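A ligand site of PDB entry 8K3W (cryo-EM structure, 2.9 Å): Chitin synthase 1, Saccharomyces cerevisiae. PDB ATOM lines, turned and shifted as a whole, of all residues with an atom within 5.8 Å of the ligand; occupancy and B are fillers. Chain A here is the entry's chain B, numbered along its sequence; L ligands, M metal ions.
The side-chain hydroxyl of Thr 453 sits at hydrogen-bond distance from an oxygen (O11) of the ligand, at 2.9 Å. O of Thr 453 lies within hydrogen-bond range of O11 of the ligand, at 2.9 Å. NE of Arg 759 lies within salt-bridge range of O16 of the ligand.
The backbone NH (N) of Gln 576 sits at hydrogen-bond distance from the side-chain carboxylate (OD2) of Asp 500 (3.0 Å). The backbone carbonyl oxygen (O) of Met 454 sits at hydrogen-bond distance from the backbone NH (N) of Asp 500 (2.8 Å). The backbone carbonyl oxygen of Leu 601 is in hydrogen-bond range of the backbone NH of Thr 453 (3.4 Å). The side-chain hydroxyl (OG1) of Thr 453 lies within hydrogen-bond range of the side-chain carboxylate (OD1) of Asp 602, at 2.5 Å. The backbone NH of Ala 603 lies within hydrogen-bond range of the backbone carbonyl oxygen of Thr 453. OD1 of Asp 500 sits close to OD1 of Asn 575 (2.7 Å). The side-chain amino group (NZ) of Lys 578 is in salt-bridge range of the side-chain carboxylate (OD2) of Asp 602, at 3.6 Å.
Residues that only touch the ligand: Asp 500 (3.1 Å), Asp 602 (3.4 Å), Pro 747 (3.6 Å), Glu 752 (3.6 Å), Tyr 455 (3.6 Å), Lys 578 (3.7 Å), Gln 756 (3.7 Å), Leu 755 (3.9 Å) and Ala 603 (3.98 Å). Hydrophobic or aromatic side chains that line the ligand: Tyr 455, Pro 747 and Leu 755. Within 4 Å of the ligand: Thr 453, Tyr 455, Asp 500, Lys 578, Asp 602, Ala 603, Pro 747, Glu 752, Leu 755, Gln 756 and Arg 759.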
ATOM      1  N   THR A 453      -9.499  21.162 -18.248  1.00  0.00           N
ATOM      2  CA  THR A 453     -10.820  20.690 -18.747  1.00  0.00           C
ATOM      3  C   THR A 453     -11.627  21.887 -19.258  1.00  0.00           C
ATOM      4  O   THR A 453     -11.757  22.863 -18.502  1.00  0.00           O
ATOM      5  CB  THR A 453     -11.572  19.927 -17.647  1.00  0.00           C
ATOM      6  OG1 THR A 453     -11.794  20.828 -16.564  1.00  0.00           O
ATOM      7  CG2 THR A 453     -10.830  18.704 -17.160  1.00  0.00           C
ATOM      8  N   MET A 454     -12.146  21.789 -20.483  1.00  0.00           N
ATOM      9  CA  MET A 454     -13.003  22.874 -21.039  1.00  0.00           C
ATOM     10  C   MET A 454     -14.262  22.250 -21.650  1.00  0.00           C
ATOM     11  O   MET A 454     -14.119  21.273 -22.402  1.00  0.00           O
ATOM     12  CB  MET A 454     -12.251  23.653 -22.131  1.00  0.00           C
ATOM     13  N   TYR A 455     -15.445  22.800 -21.337  1.00  0.00           N
ATOM     14  CA  TYR A 455     -16.710  22.303 -21.932  1.00  0.00           C
ATOM     15  C   TYR A 455     -17.233  23.364 -22.897  1.00  0.00           C
ATOM     16  O   TYR A 455     -16.961  23.259 -24.110  1.00  0.00           O
ATOM     17  CB  TYR A 455     -17.729  21.975 -20.843  1.00  0.00           C
ATOM     18  N   ASN A 456     -17.950  24.366 -22.384  1.00  0.00           N
ATOM     19  CA  ASN A 456     -18.405  25.485 -23.246  1.00  0.00           C
ATOM     20  C   ASN A 456     -17.163  26.190 -23.785  1.00  0.00           C
ATOM     21  O   ASN A 456     -17.293  26.929 -24.789  1.00  0.00           O
ATOM     22  CB  ASN A 456     -19.327  26.447 -22.486  1.00  0.00           C
ATOM     23  N   ASP A 500     -14.779  19.143 -24.096  1.00  0.00           N
ATOM     24  CA  ASP A 500     -15.846  18.106 -24.012  1.00  0.00           C
ATOM     25  C   ASP A 500     -16.535  17.960 -25.370  1.00  0.00           C
ATOM     26  O   ASP A 500     -16.689  16.802 -25.822  1.00  0.00           O
ATOM     27  CB  ASP A 500     -16.835  18.445 -22.897  1.00  0.00           C
ATOM     28  CG  ASP A 500     -17.886  17.373 -22.666  1.00  0.00           C
ATOM     29  OD1 ASP A 500     -18.701  17.539 -21.743  1.00  0.00           O
ATOM     30  OD2 ASP A 500     -17.882  16.366 -23.420  1.00  0.00           O
ATOM     31  N   ASN A 575     -20.900  15.100 -26.056  1.00  0.00           N
ATOM     32  CA  ASN A 575     -20.919  15.562 -24.662  1.00  0.00           C
ATOM     33  C   ASN A 575     -20.920  14.372 -23.702  1.00  0.00           C
ATOM     34  O   ASN A 575     -21.958  13.870 -23.271  1.00  0.00           O
ATOM     35  CB  ASN A 575     -22.098  16.467 -24.406  1.00  0.00           C
ATOM     36  CG  ASN A 575     -22.086  17.040 -23.004  1.00  0.00           C
ATOM     37  OD1 ASN A 575     -21.201  17.810 -22.652  1.00  0.00           O
ATOM     38  ND2 ASN A 575     -23.063  16.657 -22.199  1.00  0.00           N
ATOM     39  N   GLN A 576     -19.709  13.932 -23.373  1.00  0.00           N
ATOM     40  CA  GLN A 576     -19.498  13.039 -22.253  1.00  0.00           C
ATOM     41  C   GLN A 576     -18.995  13.850 -21.066  1.00  0.00           C
ATOM     42  O   GLN A 576     -18.391  14.915 -21.241  1.00  0.00           O
ATOM     43  CB  GLN A 576     -18.502  11.945 -22.629  1.00  0.00           C
ATOM     44  CG  GLN A 576     -18.957  11.157 -23.838  1.00  0.00           C
ATOM     45  CD  GLN A 576     -17.943  10.122 -24.284  1.00  0.00           C
ATOM     46  OE1 GLN A 576     -16.746  10.384 -24.296  1.00  0.00           O
ATOM     47  NE2 GLN A 576     -18.432   8.951 -24.658  1.00  0.00           N
ATOM     48  N   LYS A 577     -19.266  13.378 -19.857  1.00  0.00           N
ATOM     49  CA  LYS A 577     -19.119  14.205 -18.677  1.00  0.00           C
ATOM     50  C   LYS A 577     -17.644  14.339 -18.280  1.00  0.00           C
ATOM     51  O   LYS A 577     -16.743  13.844 -18.957  1.00  0.00           O
ATOM     52  CB  LYS A 577     -19.974  13.651 -17.540  1.00  0.00           C
ATOM     53  CG  LYS A 577     -21.461  13.771 -17.810  1.00  0.00           C
ATOM     54  CD  LYS A 577     -22.294  13.236 -16.661  1.00  0.00           C
ATOM     55  CE  LYS A 577     -23.778  13.358 -16.962  1.00  0.00           C
ATOM     56  NZ  LYS A 577     -24.638  12.836 -15.865  1.00  0.00           N
ATOM     57  N   LYS A 578     -17.402  15.028 -17.163  1.00  0.00           N
ATOM     58  CA  LYS A 578     -16.036  15.347 -16.748  1.00  0.00           C
ATOM     59  C   LYS A 578     -15.251  14.091 -16.391  1.00  0.00           C
ATOM     60  O   LYS A 578     -14.031  14.039 -16.578  1.00  0.00           O
ATOM     61  CB  LYS A 578     -16.073  16.316 -15.573  1.00  0.00           C
ATOM     62  CG  LYS A 578     -14.719  16.823 -15.135  1.00  0.00           C
ATOM     63  CD  LYS A 578     -14.866  17.901 -14.076  1.00  0.00           C
ATOM     64  CE  LYS A 578     -14.020  17.587 -12.849  1.00  0.00           C
ATOM     65  NZ  LYS A 578     -14.038  18.688 -11.853  1.00  0.00           N
ATOM     66  N   SER A 581     -13.509  12.930 -19.333  1.00  0.00           N
ATOM     67  CA  SER A 581     -12.326  13.735 -19.603  1.00  0.00           C
ATOM     68  C   SER A 581     -11.159  13.283 -18.734  1.00  0.00           C
ATOM     69  O   SER A 581     -10.028  13.153 -19.206  1.00  0.00           O
ATOM     70  CB  SER A 581     -12.632  15.204 -19.360  1.00  0.00           C
ATOM     71  OG  SER A 581     -13.757  15.626 -20.116  1.00  0.00           O
ATOM     72  N   LEU A 601      -6.464  20.949 -13.619  1.00  0.00           N
ATOM     73  CA  LEU A 601      -6.985  22.301 -13.615  1.00  0.00           C
ATOM     74  C   LEU A 601      -8.350  22.327 -14.277  1.00  0.00           C
ATOM     75  O   LEU A 601      -8.779  21.350 -14.904  1.00  0.00           O
ATOM     76  CB  LEU A 601      -6.031  23.262 -14.338  1.00  0.00           C
ATOM     77  CG  LEU A 601      -4.827  23.813 -13.591  1.00  0.00           C
ATOM     78  CD1 LEU A 601      -3.786  24.283 -14.575  1.00  0.00           C
ATOM     79  CD2 LEU A 601      -5.267  24.963 -12.733  1.00  0.00           C
ATOM     80  N   ASP A 602      -9.022  23.469 -14.168  1.00  0.00           N
ATOM     81  CA  ASP A 602     -10.341  23.660 -14.838  1.00  0.00           C
ATOM     82  C   ASP A 602     -10.324  25.031 -15.512  1.00  0.00           C
ATOM     83  O   ASP A 602      -9.842  25.984 -14.876  1.00  0.00           O
ATOM     84  CB  ASP A 602     -11.504  23.538 -13.851  1.00  0.00           C
ATOM     85  CG  ASP A 602     -11.891  22.112 -13.513  1.00  0.00           C
ATOM     86  OD1 ASP A 602     -11.313  21.187 -14.112  1.00  0.00           O
ATOM     87  OD2 ASP A 602     -12.776  21.936 -12.649  1.00  0.00           O
ATOM     88  N   ALA A 603     -10.821  25.131 -16.748  1.00  0.00           N
ATOM     89  CA  ALA A 603     -10.747  26.416 -17.484  1.00  0.00           C
ATOM     90  C   ALA A 603     -11.361  27.516 -16.622  1.00  0.00           C
ATOM     91  O   ALA A 603     -12.435  27.298 -16.045  1.00  0.00           O
ATOM     92  CB  ALA A 603     -11.452  26.286 -18.807  1.00  0.00           C
ATOM     93  N   VAL A 746     -16.638  33.107  -8.694  1.00  0.00           N
ATOM     94  CA  VAL A 746     -17.732  32.499  -7.952  1.00  0.00           C
ATOM     95  C   VAL A 746     -19.065  32.969  -8.521  1.00  0.00           C
ATOM     96  O   VAL A 746     -19.133  34.057  -9.100  1.00  0.00           O
ATOM     97  CB  VAL A 746     -17.636  32.812  -6.454  1.00  0.00           C
ATOM     98  CG1 VAL A 746     -16.334  32.282  -5.892  1.00  0.00           C
ATOM     99  CG2 VAL A 746     -17.749  34.304  -6.215  1.00  0.00           C
ATOM    100  N   PRO A 747     -20.135  32.176  -8.413  1.00  0.00           N
ATOM    101  CA  PRO A 747     -21.440  32.622  -8.895  1.00  0.00           C
ATOM    102  C   PRO A 747     -21.923  33.855  -8.140  1.00  0.00           C
ATOM    103  O   PRO A 747     -21.683  34.007  -6.951  1.00  0.00           O
ATOM    104  CB  PRO A 747     -22.341  31.419  -8.639  1.00  0.00           C
ATOM    105  CG  PRO A 747     -21.603  30.576  -7.667  1.00  0.00           C
ATOM    106  CD  PRO A 747     -20.158  30.773  -7.978  1.00  0.00           C
ATOM    107  N   GLU A 752     -27.752  30.135  -9.944  1.00  0.00           N
ATOM    108  CA  GLU A 752     -26.527  29.398 -10.230  1.00  0.00           C
ATOM    109  C   GLU A 752     -25.764  29.056  -8.968  1.00  0.00           C
ATOM    110  O   GLU A 752     -25.077  28.038  -8.937  1.00  0.00           O
ATOM    111  CB  GLU A 752     -25.636  30.180 -11.189  1.00  0.00           C
ATOM    112  CG  GLU A 752     -25.375  31.601 -10.790  1.00  0.00           C
ATOM    113  CD  GLU A 752     -25.049  32.479 -11.979  1.00  0.00           C
ATOM    114  OE1 GLU A 752     -25.905  32.583 -12.882  1.00  0.00           O
ATOM    115  OE2 GLU A 752     -23.948  33.057 -12.015  1.00  0.00           O
ATOM    116  N   PHE A 753     -25.876  29.877  -7.922  1.00  0.00           N
ATOM    117  CA  PHE A 753     -25.263  29.532  -6.638  1.00  0.00           C
ATOM    118  C   PHE A 753     -25.861  28.256  -6.072  1.00  0.00           C
ATOM    119  O   PHE A 753     -25.145  27.345  -5.642  1.00  0.00           O
ATOM    120  CB  PHE A 753     -25.432  30.697  -5.676  1.00  0.00           C
ATOM    121  CG  PHE A 753     -24.836  30.468  -4.324  1.00  0.00           C
ATOM    122  CD1 PHE A 753     -25.508  30.860  -3.183  1.00  0.00           C
ATOM    123  CD2 PHE A 753     -23.593  29.884  -4.201  1.00  0.00           C
ATOM    124  CE1 PHE A 753     -24.954  30.661  -1.944  1.00  0.00           C
ATOM    125  CE2 PHE A 753     -23.038  29.685  -2.962  1.00  0.00           C
ATOM    126  CZ  PHE A 753     -23.716  30.069  -1.832  1.00  0.00           C
ATOM    127  N   LEU A 755     -27.508  25.941  -7.783  1.00  0.00           N
ATOM    128  CA  LEU A 755     -27.180  24.832  -8.670  1.00  0.00           C
ATOM    129  C   LEU A 755     -25.740  24.360  -8.492  1.00  0.00           C
ATOM    130  O   LEU A 755     -25.470  23.167  -8.639  1.00  0.00           O
ATOM    131  CB  LEU A 755     -27.418  25.220 -10.121  1.00  0.00           C
ATOM    132  CG  LEU A 755     -28.892  25.427 -10.479  1.00  0.00           C
ATOM    133  CD1 LEU A 755     -29.017  26.309 -11.709  1.00  0.00           C
ATOM    134  CD2 LEU A 755     -29.571  24.092 -10.694  1.00  0.00           C
ATOM    135  N   GLN A 756     -24.812  25.274  -8.199  1.00  0.00           N
ATOM    136  CA  GLN A 756     -23.437  24.862  -7.947  1.00  0.00           C
ATOM    137  C   GLN A 756     -23.324  24.103  -6.637  1.00  0.00           C
ATOM    138  O   GLN A 756     -22.682  23.041  -6.579  1.00  0.00           O
ATOM    139  CB  GLN A 756     -22.517  26.074  -7.946  1.00  0.00           C
ATOM    140  CG  GLN A 756     -21.157  25.785  -7.341  1.00  0.00           C
ATOM    141  CD  GLN A 756     -20.290  27.015  -7.232  1.00  0.00           C
ATOM    142  OE1 GLN A 756     -20.534  27.893  -6.404  1.00  0.00           O
ATOM    143  NE2 GLN A 756     -19.262  27.086  -8.057  1.00  0.00           N
ATOM    144  N   ARG A 759     -24.167  20.184  -6.154  1.00  0.00           N
ATOM    145  CA  ARG A 759     -23.208  19.097  -6.477  1.00  0.00           C
ATOM    146  C   ARG A 759     -22.190  18.976  -5.335  1.00  0.00           C
ATOM    147  O   ARG A 759     -21.732  17.839  -5.092  1.00  0.00           O
ATOM    148  CB  ARG A 759     -22.517  19.399  -7.801  1.00  0.00           C
ATOM    149  CG  ARG A 759     -23.428  19.997  -8.858  1.00  0.00           C
ATOM    150  CD  ARG A 759     -22.813  19.949 -10.251  1.00  0.00           C
ATOM    151  NE  ARG A 759     -21.406  20.327 -10.248  1.00  0.00           N
ATOM    152  CZ  ARG A 759     -20.403  19.467 -10.181  1.00  0.00           C
ATOM    153  NH1 ARG A 759     -20.635  18.171 -10.099  1.00  0.00           N
ATOM    154  NH2 ARG A 759     -19.147  19.905 -10.190  1.00  0.00           N
ATOM    155  N   TRP A 760     -21.855  20.080  -4.674  1.00  0.00           N
ATOM    156  CA  TRP A 760     -20.921  20.031  -3.558  1.00  0.00           C
ATOM    157  C   TRP A 760     -21.536  19.301  -2.374  1.00  0.00           C
ATOM    158  O   TRP A 760     -20.883  18.443  -1.761  1.00  0.00           O
ATOM    159  CB  TRP A 760     -20.503  21.430  -3.122  1.00  0.00           C
ATOM    160  CG  TRP A 760     -19.822  22.247  -4.157  1.00  0.00           C
ATOM    161  CD1 TRP A 760     -19.825  22.052  -5.504  1.00  0.00           C
ATOM    162  CD2 TRP A 760     -18.981  23.383  -3.921  1.00  0.00           C
ATOM    163  NE1 TRP A 760     -19.064  23.003  -6.120  1.00  0.00           N
ATOM    164  CE2 TRP A 760     -18.528  23.833  -5.171  1.00  0.00           C
ATOM    165  CE3 TRP A 760     -18.579  24.065  -2.769  1.00  0.00           C
ATOM    166  CZ2 TRP A 760     -17.699  24.937  -5.301  1.00  0.00           C
ATOM    167  CZ3 TRP A 760     -17.750  25.154  -2.907  1.00  0.00           C
ATOM    168  CH2 TRP A 760     -17.321  25.586  -4.160  1.00  0.00           C
HETATM  169  C1  LIG L   1     -22.487  24.840 -11.479  1.00  0.00           C
HETATM  170  C2  LIG L   1     -23.793  24.849 -12.290  1.00  0.00           C
HETATM  171  C3  LIG L   1     -23.844  25.866 -13.421  1.00  0.00           C
HETATM  172  C4  LIG L   1     -22.755  26.952 -13.549  1.00  0.00           C
HETATM  173  C5  LIG L   1     -21.863  27.080 -12.321  1.00  0.00           C
HETATM  174  C6  LIG L   1     -22.426  28.083 -11.342  1.00  0.00           C
HETATM  175  C7  LIG L   1     -25.496  23.465 -13.289  1.00  0.00           C
HETATM  176  C8  LIG L   1     -26.296  22.230 -13.326  1.00  0.00           C
HETATM  177  N1  LIG L   1     -24.271  23.548 -12.794  1.00  0.00           N
HETATM  178  O1  LIG L   1     -21.779  23.603 -11.369  1.00  0.00           O
HETATM  179  O2  LIG L   1     -25.159  26.470 -13.398  1.00  0.00           O
HETATM  180  O3  LIG L   1     -21.980  26.889 -14.789  1.00  0.00           O
HETATM  181  O4  LIG L   1     -21.528  25.828 -11.773  1.00  0.00           O
HETATM  182  O5  LIG L   1     -21.487  29.163 -11.258  1.00  0.00           O
HETATM  183  O6  LIG L   1     -26.070  24.403 -13.727  1.00  0.00           O
HETATM  184  N2  LIG L   1     -17.085  20.305 -17.550  1.00  0.00           N
HETATM  185  C9  LIG L   1     -18.345  20.392 -17.000  1.00  0.00           C
HETATM  186  N3  LIG L   1     -19.350  19.642 -17.389  1.00  0.00           N
HETATM  187  C10 LIG L   1     -19.181  18.783 -18.305  1.00  0.00           C
HETATM  188  C11 LIG L   1     -17.938  18.622 -18.888  1.00  0.00           C
HETATM  189  C12 LIG L   1     -16.876  19.407 -18.469  1.00  0.00           C
HETATM  190  O7  LIG L   1     -18.564  21.210 -16.143  1.00  0.00           O
HETATM  191  O8  LIG L   1     -20.165  18.127 -18.611  1.00  0.00           O
HETATM  192  C13 LIG L   1     -16.038  21.183 -17.058  1.00  0.00           C
HETATM  193  C14 LIG L   1     -16.239  22.649 -16.839  1.00  0.00           C
HETATM  194  O9  LIG L   1     -16.069  23.760 -17.737  1.00  0.00           O
HETATM  195  C15 LIG L   1     -15.163  22.920 -15.884  1.00  0.00           C
HETATM  196  C16 LIG L   1     -15.359  21.831 -14.914  1.00  0.00           C
HETATM  197  O10 LIG L   1     -16.083  20.938 -15.703  1.00  0.00           O
HETATM  198  O11 LIG L   1     -13.974  22.708 -16.609  1.00  0.00           O
HETATM  199  C17 LIG L   1     -16.233  22.317 -13.773  1.00  0.00           C
HETATM  200  O12 LIG L   1     -17.638  22.226 -14.011  1.00  0.00           O
HETATM  201  P1  LIG L   1     -18.797  23.307 -13.721  1.00  0.00           P
HETATM  202  O13 LIG L   1     -19.732  23.170 -14.864  1.00  0.00           O
HETATM  203  O14 LIG L   1     -18.223  24.618 -13.424  1.00  0.00           O
HETATM  204  O15 LIG L   1     -19.597  22.767 -12.445  1.00  0.00           O
HETATM  205  P2  LIG L   1     -20.175  23.509 -11.103  1.00  0.00           P
HETATM  206  O16 LIG L   1     -19.989  22.399 -10.117  1.00  0.00           O
HETATM  207  O17 LIG L   1     -19.350  24.767 -11.011  1.00  0.00           O
HETATM  208 MG    MG M   1     -15.813  27.228 -13.944  1.00  0.00          MG
